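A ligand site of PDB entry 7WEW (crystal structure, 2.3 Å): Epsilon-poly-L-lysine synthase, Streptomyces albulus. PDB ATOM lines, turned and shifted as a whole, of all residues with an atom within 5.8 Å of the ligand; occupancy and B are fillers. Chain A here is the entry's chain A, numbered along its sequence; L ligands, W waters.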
ATOM      1  N   THR A 165      -3.883 -23.189  19.530  1.00  0.00           N
ATOM      2  CA  THR A 165      -2.622 -23.891  19.339  1.00  0.00           C
ATOM      3  C   THR A 165      -2.921 -25.332  18.965  1.00  0.00           C
ATOM      4  O   THR A 165      -3.672 -26.012  19.676  1.00  0.00           O
ATOM      5  CB  THR A 165      -1.759 -23.797  20.596  1.00  0.00           C
ATOM      6  OG1 THR A 165      -0.451 -24.320  20.317  1.00  0.00           O
ATOM      7  CG2 THR A 165      -2.399 -24.551  21.763  1.00  0.00           C
ATOM      8  N   SER A 166      -2.320 -25.798  17.856  1.00  0.00           N
ATOM      9  CA  SER A 166      -2.695 -27.064  17.246  1.00  0.00           C
ATOM     10  C   SER A 166      -2.671 -28.226  18.243  1.00  0.00           C
ATOM     11  O   SER A 166      -3.549 -29.094  18.226  1.00  0.00           O
ATOM     12  CB  SER A 166      -1.791 -27.364  16.046  1.00  0.00           C
ATOM     13  OG  SER A 166      -0.441 -27.038  16.341  1.00  0.00           O
ATOM     14  N   GLU A 189       9.943  -7.986  27.242  1.00  0.00           N
ATOM     15  CA  GLU A 189      10.845  -7.915  26.109  1.00  0.00           C
ATOM     16  C   GLU A 189      11.524  -6.562  25.980  1.00  0.00           C
ATOM     17  O   GLU A 189      12.588  -6.466  25.369  1.00  0.00           O
ATOM     18  CB  GLU A 189      10.125  -8.254  24.809  1.00  0.00           C
ATOM     19  CG  GLU A 189       9.721  -9.725  24.720  1.00  0.00           C
ATOM     20  CD  GLU A 189       9.457 -10.171  23.282  1.00  0.00           C
ATOM     21  OE1 GLU A 189       8.984  -9.324  22.487  1.00  0.00           O
ATOM     22  OE2 GLU A 189       9.738 -11.351  22.942  1.00  0.00           O
ATOM     23  N   PHE A 213      -0.981 -17.018  14.757  1.00  0.00           N
ATOM     24  CA  PHE A 213       0.168 -17.527  15.488  1.00  0.00           C
ATOM     25  C   PHE A 213       0.684 -16.423  16.396  1.00  0.00           C
ATOM     26  O   PHE A 213       0.963 -15.310  15.924  1.00  0.00           O
ATOM     27  CB  PHE A 213       1.252 -17.985  14.503  1.00  0.00           C
ATOM     28  CG  PHE A 213       2.487 -18.548  15.147  1.00  0.00           C
ATOM     29  CD1 PHE A 213       2.395 -19.566  16.081  1.00  0.00           C
ATOM     30  CD2 PHE A 213       3.739 -18.079  14.786  1.00  0.00           C
ATOM     31  CE1 PHE A 213       3.534 -20.089  16.664  1.00  0.00           C
ATOM     32  CE2 PHE A 213       4.878 -18.602  15.369  1.00  0.00           C
ATOM     33  CZ  PHE A 213       4.780 -19.612  16.302  1.00  0.00           C
ATOM     34  N   ASP A 214       0.812 -16.702  17.695  1.00  0.00           N
ATOM     35  CA  ASP A 214       1.004 -15.592  18.635  1.00  0.00           C
ATOM     36  C   ASP A 214       2.369 -14.917  18.526  1.00  0.00           C
ATOM     37  O   ASP A 214       2.556 -13.847  19.121  1.00  0.00           O
ATOM     38  CB  ASP A 214       0.727 -16.047  20.076  1.00  0.00           C
ATOM     39  CG  ASP A 214       1.867 -16.827  20.704  1.00  0.00           C
ATOM     40  OD1 ASP A 214       2.836 -17.203  20.009  1.00  0.00           O
ATOM     41  OD2 ASP A 214       1.795 -17.054  21.938  1.00  0.00           O
ATOM     42  N   ALA A 215       3.317 -15.470  17.761  1.00  0.00           N
ATOM     43  CA  ALA A 215       4.538 -14.710  17.488  1.00  0.00           C
ATOM     44  C   ALA A 215       4.241 -13.408  16.756  1.00  0.00           C
ATOM     45  O   ALA A 215       5.058 -12.468  16.833  1.00  0.00           O
ATOM     46  CB  ALA A 215       5.517 -15.563  16.651  1.00  0.00           C
ATOM     47  N   GLU A 218       4.334 -10.633  19.046  1.00  0.00           N
ATOM     48  CA  GLU A 218       5.670 -10.073  19.230  1.00  0.00           C
ATOM     49  C   GLU A 218       5.980  -9.039  18.145  1.00  0.00           C
ATOM     50  O   GLU A 218       6.475  -7.948  18.444  1.00  0.00           O
ATOM     51  CB  GLU A 218       6.699 -11.178  19.256  1.00  0.00           C
ATOM     52  CG  GLU A 218       8.098 -10.677  19.488  1.00  0.00           C
ATOM     53  CD  GLU A 218       9.040 -11.823  19.595  1.00  0.00           C
ATOM     54  OE1 GLU A 218       9.305 -12.468  18.550  1.00  0.00           O
ATOM     55  OE2 GLU A 218       9.480 -12.110  20.721  1.00  0.00           O
ATOM     56  N   SER A 257      11.182 -10.729  13.113  1.00  0.00           N
ATOM     57  CA  SER A 257      10.837 -11.834  14.001  1.00  0.00           C
ATOM     58  C   SER A 257      10.235 -12.929  13.141  1.00  0.00           C
ATOM     59  O   SER A 257       9.284 -12.674  12.397  1.00  0.00           O
ATOM     60  CB  SER A 257       9.864 -11.386  15.098  1.00  0.00           C
ATOM     61  OG  SER A 257       9.531 -12.474  15.930  1.00  0.00           O
ATOM     62  N   THR A 258      10.811 -14.119  13.201  1.00  0.00           N
ATOM     63  CA  THR A 258      10.425 -15.151  12.253  1.00  0.00           C
ATOM     64  C   THR A 258      10.618 -16.531  12.882  1.00  0.00           C
ATOM     65  O   THR A 258      10.867 -16.673  14.085  1.00  0.00           O
ATOM     66  CB  THR A 258      11.216 -15.003  10.947  1.00  0.00           C
ATOM     67  OG1 THR A 258      10.639 -15.848   9.946  1.00  0.00           O
ATOM     68  CG2 THR A 258      12.644 -15.430  11.142  1.00  0.00           C
ATOM     69  N   ILE A 278      15.006 -12.126  15.464  1.00  0.00           N
ATOM     70  CA  ILE A 278      14.461 -13.014  16.470  1.00  0.00           C
ATOM     71  C   ILE A 278      13.911 -14.266  15.769  1.00  0.00           C
ATOM     72  O   ILE A 278      13.185 -14.140  14.772  1.00  0.00           O
ATOM     73  CB  ILE A 278      13.342 -12.325  17.274  1.00  0.00           C
ATOM     74  CG1 ILE A 278      13.927 -11.170  18.081  1.00  0.00           C
ATOM     75  CG2 ILE A 278      12.582 -13.351  18.172  1.00  0.00           C
ATOM     76  CD1 ILE A 278      12.977 -10.055  18.284  1.00  0.00           C
ATOM     77  N   VAL A 279      14.259 -15.450  16.278  1.00  0.00           N
ATOM     78  CA  VAL A 279      13.642 -16.697  15.823  1.00  0.00           C
ATOM     79  C   VAL A 279      12.958 -17.379  17.010  1.00  0.00           C
ATOM     80  O   VAL A 279      13.386 -17.240  18.163  1.00  0.00           O
ATOM     81  CB  VAL A 279      14.664 -17.641  15.155  1.00  0.00           C
ATOM     82  CG1 VAL A 279      15.142 -17.027  13.840  1.00  0.00           C
ATOM     83  CG2 VAL A 279      15.841 -17.915  16.111  1.00  0.00           C
ATOM     84  N   GLY A 280      11.868 -18.092  16.734  1.00  0.00           N
ATOM     85  CA  GLY A 280      11.199 -18.856  17.767  1.00  0.00           C
ATOM     86  C   GLY A 280      10.233 -19.847  17.174  1.00  0.00           C
ATOM     87  O   GLY A 280      10.030 -19.913  15.958  1.00  0.00           O
ATOM     88  N   GLY A 281       9.620 -20.635  18.062  1.00  0.00           N
ATOM     89  CA  GLY A 281       8.583 -21.557  17.646  1.00  0.00           C
ATOM     90  C   GLY A 281       9.029 -22.971  17.364  1.00  0.00           C
ATOM     91  O   GLY A 281       8.215 -23.885  17.456  1.00  0.00           O
ATOM     92  N   GLU A 282      10.304 -23.175  16.981  1.00  0.00           N
ATOM     93  CA  GLU A 282      10.893 -24.497  16.771  1.00  0.00           C
ATOM     94  C   GLU A 282      12.407 -24.339  16.896  1.00  0.00           C
ATOM     95  O   GLU A 282      12.917 -23.235  17.048  1.00  0.00           O
ATOM     96  CB  GLU A 282      10.507 -25.096  15.413  1.00  0.00           C
ATOM     97  CG  GLU A 282      10.639 -24.098  14.281  1.00  0.00           C
ATOM     98  CD  GLU A 282      10.318 -24.665  12.910  1.00  0.00           C
ATOM     99  OE1 GLU A 282       9.563 -25.656  12.820  1.00  0.00           O
ATOM    100  OE2 GLU A 282      10.817 -24.098  11.923  1.00  0.00           O
ATOM    101  N   SER A 283      13.119 -25.467  16.849  1.00  0.00           N
ATOM    102  CA  SER A 283      14.547 -25.447  17.137  1.00  0.00           C
ATOM    103  C   SER A 283      15.287 -24.636  16.094  1.00  0.00           C
ATOM    104  O   SER A 283      15.071 -24.799  14.889  1.00  0.00           O
ATOM    105  CB  SER A 283      15.109 -26.866  17.191  1.00  0.00           C
ATOM    106  OG  SER A 283      14.509 -27.643  18.206  1.00  0.00           O
ATOM    107  N   CYS A 284      16.172 -23.764  16.549  1.00  0.00           N
ATOM    108  CA  CYS A 284      16.984 -22.967  15.633  1.00  0.00           C
ATOM    109  C   CYS A 284      18.233 -23.755  15.231  1.00  0.00           C
ATOM    110  O   CYS A 284      19.060 -24.074  16.101  1.00  0.00           O
ATOM    111  CB  CYS A 284      17.357 -21.640  16.265  1.00  0.00           C
ATOM    112  SG  CYS A 284      18.447 -20.650  15.233  1.00  0.00           S
ATOM    113  N   ASN A 301      17.261 -16.248  20.213  1.00  0.00           N
ATOM    114  CA  ASN A 301      16.364 -17.383  20.241  1.00  0.00           C
ATOM    115  C   ASN A 301      15.277 -17.099  21.285  1.00  0.00           C
ATOM    116  O   ASN A 301      15.555 -16.559  22.364  1.00  0.00           O
ATOM    117  CB  ASN A 301      17.135 -18.650  20.591  1.00  0.00           C
ATOM    118  CG  ASN A 301      16.407 -19.910  20.191  1.00  0.00           C
ATOM    119  OD1 ASN A 301      15.341 -19.851  19.576  1.00  0.00           O
ATOM    120  ND2 ASN A 301      16.990 -21.053  20.512  1.00  0.00           N
ATOM    121  N   THR A 302      14.042 -17.420  20.936  1.00  0.00           N
ATOM    122  CA  THR A 302      12.909 -17.246  21.848  1.00  0.00           C
ATOM    123  C   THR A 302      12.158 -18.559  21.918  1.00  0.00           C
ATOM    124  O   THR A 302      11.877 -19.161  20.876  1.00  0.00           O
ATOM    125  CB  THR A 302      11.970 -16.117  21.385  1.00  0.00           C
ATOM    126  OG1 THR A 302      11.623 -16.317  20.013  1.00  0.00           O
ATOM    127  CG2 THR A 302      12.594 -14.717  21.561  1.00  0.00           C
ATOM    128  N   TYR A 303      11.814 -18.996  23.127  1.00  0.00           N
ATOM    129  CA  TYR A 303      11.020 -20.195  23.349  1.00  0.00           C
ATOM    130  C   TYR A 303       9.787 -19.871  24.190  1.00  0.00           C
ATOM    131  O   TYR A 303       9.856 -19.100  25.148  1.00  0.00           O
ATOM    132  CB  TYR A 303      11.843 -21.303  24.047  1.00  0.00           C
ATOM    133  CG  TYR A 303      10.982 -22.359  24.676  1.00  0.00           C
ATOM    134  CD1 TYR A 303      10.342 -22.144  25.897  1.00  0.00           C
ATOM    135  CD2 TYR A 303      10.770 -23.589  24.040  1.00  0.00           C
ATOM    136  CE1 TYR A 303       9.525 -23.112  26.453  1.00  0.00           C
ATOM    137  CE2 TYR A 303       9.963 -24.574  24.599  1.00  0.00           C
ATOM    138  CZ  TYR A 303       9.358 -24.321  25.804  1.00  0.00           C
ATOM    139  OH  TYR A 303       8.556 -25.278  26.373  1.00  0.00           O
ATOM    140  N   GLY A 304       8.666 -20.498  23.855  1.00  0.00           N
ATOM    141  CA  GLY A 304       7.486 -20.366  24.687  1.00  0.00           C
ATOM    142  C   GLY A 304       6.266 -20.991  24.070  1.00  0.00           C
ATOM    143  O   GLY A 304       6.038 -20.944  22.852  1.00  0.00           O
ATOM    144  N   PRO A 305       5.434 -21.606  24.909  1.00  0.00           N
ATOM    145  CA  PRO A 305       4.141 -22.090  24.430  1.00  0.00           C
ATOM    146  C   PRO A 305       3.110 -20.961  24.417  1.00  0.00           C
ATOM    147  O   PRO A 305       3.205 -19.988  25.173  1.00  0.00           O
ATOM    148  CB  PRO A 305       3.775 -23.179  25.454  1.00  0.00           C
ATOM    149  CG  PRO A 305       4.412 -22.705  26.729  1.00  0.00           C
ATOM    150  CD  PRO A 305       5.651 -21.902  26.342  1.00  0.00           C
ATOM    151  N   THR A 306       2.133 -21.088  23.517  1.00  0.00           N
ATOM    152  CA  THR A 306       1.006 -20.168  23.519  1.00  0.00           C
ATOM    153  C   THR A 306       0.381 -20.071  24.907  1.00  0.00           C
ATOM    154  O   THR A 306      -0.081 -18.989  25.304  1.00  0.00           O
ATOM    155  CB  THR A 306      -0.066 -20.614  22.497  1.00  0.00           C
ATOM    156  OG1 THR A 306       0.514 -20.764  21.191  1.00  0.00           O
ATOM    157  CG2 THR A 306      -1.198 -19.589  22.414  1.00  0.00           C
ATOM    158  N   GLU A 307       0.417 -21.172  25.672  1.00  0.00           N
ATOM    159  CA  GLU A 307      -0.200 -21.258  26.995  1.00  0.00           C
ATOM    160  C   GLU A 307       0.466 -20.352  28.054  1.00  0.00           C
ATOM    161  O   GLU A 307      -0.146 -20.100  29.105  1.00  0.00           O
ATOM    162  CB  GLU A 307      -0.181 -22.716  27.478  1.00  0.00           C
ATOM    163  CG  GLU A 307      -1.083 -23.710  26.705  1.00  0.00           C
ATOM    164  CD  GLU A 307      -0.509 -24.166  25.387  1.00  0.00           C
ATOM    165  OE1 GLU A 307       0.539 -23.612  24.962  1.00  0.00           O
ATOM    166  OE2 GLU A 307      -1.110 -25.072  24.758  1.00  0.00           O
ATOM    167  N   THR A 309       1.914 -17.201  27.101  1.00  0.00           N
ATOM    168  CA  THR A 309       1.965 -15.887  26.470  1.00  0.00           C
ATOM    169  C   THR A 309       3.228 -15.637  25.650  1.00  0.00           C
ATOM    170  O   THR A 309       4.118 -14.866  26.052  1.00  0.00           O
ATOM    171  CB  THR A 309       1.819 -14.777  27.503  1.00  0.00           C
ATOM    172  OG1 THR A 309       0.595 -14.937  28.217  1.00  0.00           O
ATOM    173  CG2 THR A 309       1.803 -13.430  26.815  1.00  0.00           C
ATOM    174  N   VAL A 310       3.302 -16.282  24.490  1.00  0.00           N
ATOM    175  CA  VAL A 310       4.240 -15.970  23.418  1.00  0.00           C
ATOM    176  C   VAL A 310       5.640 -16.481  23.724  1.00  0.00           C
ATOM    177  O   VAL A 310       6.104 -17.428  23.092  1.00  0.00           O
ATOM    178  CB  VAL A 310       4.246 -14.466  23.089  1.00  0.00           C
ATOM    179  CG1 VAL A 310       4.929 -14.221  21.749  1.00  0.00           C
ATOM    180  CG2 VAL A 310       2.812 -13.908  23.036  1.00  0.00           C
ATOM    181  N   VAL A 311       6.330 -15.852  24.671  1.00  0.00           N
ATOM    182  CA  VAL A 311       7.742 -16.166  24.951  1.00  0.00           C
ATOM    183  C   VAL A 311       7.930 -16.326  26.442  1.00  0.00           C
ATOM    184  O   VAL A 311       7.534 -15.460  27.230  1.00  0.00           O
ATOM    185  CB  VAL A 311       8.696 -15.069  24.444  1.00  0.00           C
ATOM    186  CG1 VAL A 311      10.135 -15.391  24.887  1.00  0.00           C
ATOM    187  CG2 VAL A 311       8.583 -14.918  22.930  1.00  0.00           C
ATOM    188  N   ILE A 325      17.885 -22.016  24.384  1.00  0.00           N
ATOM    189  CA  ILE A 325      16.625 -21.294  24.500  1.00  0.00           C
ATOM    190  C   ILE A 325      16.664 -20.331  25.675  1.00  0.00           C
ATOM    191  O   ILE A 325      15.874 -19.376  25.704  1.00  0.00           O
ATOM    192  CB  ILE A 325      15.402 -22.231  24.596  1.00  0.00           C
ATOM    193  CG1 ILE A 325      15.445 -23.160  25.821  1.00  0.00           C
ATOM    194  CG2 ILE A 325      15.290 -23.057  23.324  1.00  0.00           C
ATOM    195  CD1 ILE A 325      14.108 -23.966  26.063  1.00  0.00           C
ATOM    196  N   THR A 386       4.945 -28.244  30.027  1.00  0.00           N
ATOM    197  CA  THR A 386       5.133 -27.983  28.603  1.00  0.00           C
ATOM    198  C   THR A 386       5.117 -29.252  27.779  1.00  0.00           C
ATOM    199  O   THR A 386       4.785 -29.209  26.588  1.00  0.00           O
ATOM    200  CB  THR A 386       6.456 -27.246  28.348  1.00  0.00           C
ATOM    201  OG1 THR A 386       7.548 -28.135  28.629  1.00  0.00           O
ATOM    202  CG2 THR A 386       6.575 -26.008  29.205  1.00  0.00           C
ATOM    203  N   ASP A 388       7.981 -30.538  27.037  1.00  0.00           N
ATOM    204  CA  ASP A 388       9.269 -30.429  26.356  1.00  0.00           C
ATOM    205  C   ASP A 388      10.408 -30.895  27.266  1.00  0.00           C
ATOM    206  O   ASP A 388      10.458 -30.536  28.451  1.00  0.00           O
ATOM    207  CB  ASP A 388       9.573 -28.996  25.917  1.00  0.00           C
ATOM    208  CG  ASP A 388       8.570 -28.460  24.887  1.00  0.00           C
ATOM    209  OD1 ASP A 388       8.226 -29.192  23.941  1.00  0.00           O
ATOM    210  OD2 ASP A 388       8.137 -27.294  25.059  1.00  0.00           O
ATOM    211  N   PHE A 399      17.203 -26.751  24.527  1.00  0.00           N
ATOM    212  CA  PHE A 399      16.066 -27.563  24.125  1.00  0.00           C
ATOM    213  C   PHE A 399      16.526 -28.942  23.643  1.00  0.00           C
ATOM    214  O   PHE A 399      17.486 -29.052  22.868  1.00  0.00           O
ATOM    215  CB  PHE A 399      15.277 -26.866  23.035  1.00  0.00           C
ATOM    216  CG  PHE A 399      14.049 -27.604  22.613  1.00  0.00           C
ATOM    217  CD1 PHE A 399      12.860 -27.471  23.311  1.00  0.00           C
ATOM    218  CD2 PHE A 399      14.083 -28.411  21.497  1.00  0.00           C
ATOM    219  CE1 PHE A 399      11.721 -28.147  22.901  1.00  0.00           C
ATOM    220  CE2 PHE A 399      12.956 -29.100  21.100  1.00  0.00           C
ATOM    221  CZ  PHE A 399      11.762 -28.959  21.796  1.00  0.00           C
ATOM    222  N   LYS A 496       6.276 -22.832  11.151  1.00  0.00           N
ATOM    223  CA  LYS A 496       7.043 -24.017  11.515  1.00  0.00           C
ATOM    224  C   LYS A 496       6.948 -25.055  10.401  1.00  0.00           C
ATOM    225  O   LYS A 496       6.043 -25.026   9.561  1.00  0.00           O
ATOM    226  CB  LYS A 496       6.521 -24.635  12.812  1.00  0.00           C
ATOM    227  CG  LYS A 496       6.462 -23.697  14.009  1.00  0.00           C
ATOM    228  CD  LYS A 496       5.786 -24.404  15.169  1.00  0.00           C
ATOM    229  CE  LYS A 496       5.528 -23.426  16.294  1.00  0.00           C
ATOM    230  NZ  LYS A 496       5.165 -24.158  17.525  1.00  0.00           N
HETATM  231  N1  LIG L   1       4.672 -18.980  21.414  1.00  0.00           N
HETATM  232  C1  LIG L   1       5.052 -19.511  20.125  1.00  0.00           C
HETATM  233  C2  LIG L   1       6.495 -19.060  19.796  1.00  0.00           C
HETATM  234  C3  LIG L   1       6.644 -17.543  20.034  1.00  0.00           C
HETATM  235  C4  LIG L   1       7.964 -17.055  19.427  1.00  0.00           C
HETATM  236  C5  LIG L   1       7.965 -15.530  19.317  1.00  0.00           C
HETATM  237  N2  LIG L   1       9.272 -15.086  18.812  1.00  0.00           N
HETATM  238  C6  LIG L   1       4.923 -21.023  20.070  1.00  0.00           C
HETATM  239  O1  LIG L   1       5.716 -21.630  19.449  1.00  0.00           O
HETATM  240  P1  LIG L   1       3.166 -23.044  20.218  1.00  0.00           P
HETATM  241  O2  LIG L   1       4.324 -24.280  20.387  1.00  0.00           O
HETATM  242  C7  LIG L   1       5.368 -24.167  21.382  1.00  0.00           C
HETATM  243  C8  LIG L   1       6.146 -25.349  21.187  1.00  0.00           C
HETATM  244  O3  LIG L   1       7.152 -25.310  20.020  1.00  0.00           O
HETATM  245  C9  LIG L   1       8.317 -25.605  20.469  1.00  0.00           C
HETATM  246  N3  LIG L   1       9.170 -24.428  20.484  1.00  0.00           N
HETATM  247  C10 LIG L   1      10.493 -24.474  20.349  1.00  0.00           C
HETATM  248  N4  LIG L   1      11.415 -25.641  20.189  1.00  0.00           N
HETATM  249  C11 LIG L   1      12.835 -25.388  20.071  1.00  0.00           C
HETATM  250  N5  LIG L   1      13.351 -24.048  20.127  1.00  0.00           N
HETATM  251  C12 LIG L   1      12.451 -22.940  20.281  1.00  0.00           C
HETATM  252  N6  LIG L   1      12.987 -21.580  20.323  1.00  0.00           N
HETATM  253  C13 LIG L   1      10.964 -23.191  20.411  1.00  0.00           C
HETATM  254  N7  LIG L   1       9.940 -22.372  20.553  1.00  0.00           N
HETATM  255  C14 LIG L   1       8.808 -23.139  20.617  1.00  0.00           C
HETATM  256  C15 LIG L   1       8.026 -26.306  21.934  1.00  0.00           C
HETATM  257  O4  LIG L   1       7.708 -27.716  21.644  1.00  0.00           O
HETATM  258  C16 LIG L   1       7.053 -25.712  22.408  1.00  0.00           C
HETATM  259  O5  LIG L   1       6.296 -26.621  23.360  1.00  0.00           O
HETATM  260  O6  LIG L   1       2.702 -22.883  18.777  1.00  0.00           O
HETATM  261  O7  LIG L   1       2.007 -23.377  21.148  1.00  0.00           O
HETATM  262  O8  LIG L   1       3.854 -21.629  20.739  1.00  0.00           O
HETATM  263  O   HOH W   1       7.938 -30.699  21.858  1.00  0.00           O
HETATM  264  O   HOH W   2       1.683 -24.999  23.093  1.00  0.00           O
HETATM  265  O   HOH W   3       3.484 -26.931  25.375  1.00  0.00           O
HETATM  266  O   HOH W   4       9.349 -15.479  15.888  1.00  0.00           O
HETATM  267  O   HOH W   5      15.993 -23.730  19.560  1.00  0.00           O
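The side-chain carboxylate of Asp 388 sits at hydrogen-bond distance from an oxygen (O5) of the ligand, 2.6 Å away. OE1 of Glu 218 is in salt-bridge range of N2 of the ligand (2.6 Å). N1 of the ligand sits at hydrogen-bond distance from O of Val 310 (2.7 Å). A nitrogen (N6) of the ligand is in hydrogen-bond range of the backbone carbonyl oxygen (O) of Thr 302 (2.7 Å). The side-chain hydroxyl (OG1) of Thr 302 sits at hydrogen-bond distance from a nitrogen (N2) of the ligand, at 2.9 Å. The side-chain hydroxyl of Thr 165 lies within hydrogen-bond range of an oxygen (O7) of the ligand, 2.8 Å away. N1 of the ligand sits at hydrogen-bond distance from O of Gly 304. The side-chain carboxylate of Asp 214 lies within salt-bridge range of a nitrogen (N1) of the ligand, 2.9 Å away. An oxygen (O6) of the ligand lies within salt-bridge range of the side-chain amino group of Lys 496, at 3.0 Å. The backbone NH (N) of Thr 306 lies within hydrogen-bond range of an oxygen (O7) of the ligand. An oxygen (O7) of the ligand sits at hydrogen-bond distance from the side-chain hydroxyl (OG1) of Thr 306 (3.0 Å). A nitrogen (N6) of the ligand sits at hydrogen-bond distance from the side-chain amide oxygen (OD1) of Asn 301, 3.0 Å away. The backbone NH of Gly 281 sits at hydrogen-bond distance from a nitrogen (N7) of the ligand (3.1 Å).
The side-chain hydroxyl (OH) of Tyr 303 is in hydrogen-bond range of the side-chain carboxylate (OD2) of Asp 388 (2.4 Å). N of Asp 388 is in hydrogen-bond range of OG1 of Thr 386. The side-chain carboxylate (OE1) of Glu 218 sits at hydrogen-bond distance from the side-chain hydroxyl (OG) of Ser 257 (2.6 Å). The backbone NH (N) of Val 310 sits close to the side-chain carboxylate (OD2) of Asp 214, at 3.1 Å. OG1 of Thr 302 is in hydrogen-bond range of O of Val 279 (2.7 Å). O of Gly 281 lies close to NZ of Lys 496, at 3.1 Å. The backbone carbonyl oxygen (O) of Ile 278 sits at hydrogen-bond distance from the backbone NH (N) of Thr 258 (2.8 Å).
O of Glu 282 lies close to N5 of the ligand (3.2 Å). Merely in contact with the ligand: Ser 283 (3.2 Å), Phe 399 (3.6 Å), Phe 213 (3.6 Å), Ala 215 (3.6 Å), Tyr 303 (3.7 Å), Val 311 (3.7 Å), Pro 305 (3.7 Å), Ile 278 (3.8 Å), Ile 325 (3.9 Å) and Ser 257 (3.9 Å). Of the 31 residues printed, 22 come within 4 Å of the ligand.
Water W2 lies within hydrogen-bond range of an oxygen (O7) of the ligand (2.6 Å) and the side-chain carboxylate (OE1) of Glu 307 (2.6 Å). Water W5 lies within hydrogen-bond range of N5 of the ligand (2.7 Å), ND2 of Asn 301 (3.0 Å) and N of Cys 284 (3.0 Å). Water W4 lies within hydrogen-bond range of O of Thr 258 (2.6 Å), N2 of the ligand (3.0 Å) and OG of Ser 257 (3.0 Å). Water W1 lies within hydrogen-bond range of the side-chain carboxylate (OD1) of Asp 388 (2.6 Å) and an oxygen (O4) of the ligand (3.0 Å). Water W3 bridges the backbone carbonyl oxygen of Thr 386 and an oxygen (O5) of the ligand.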
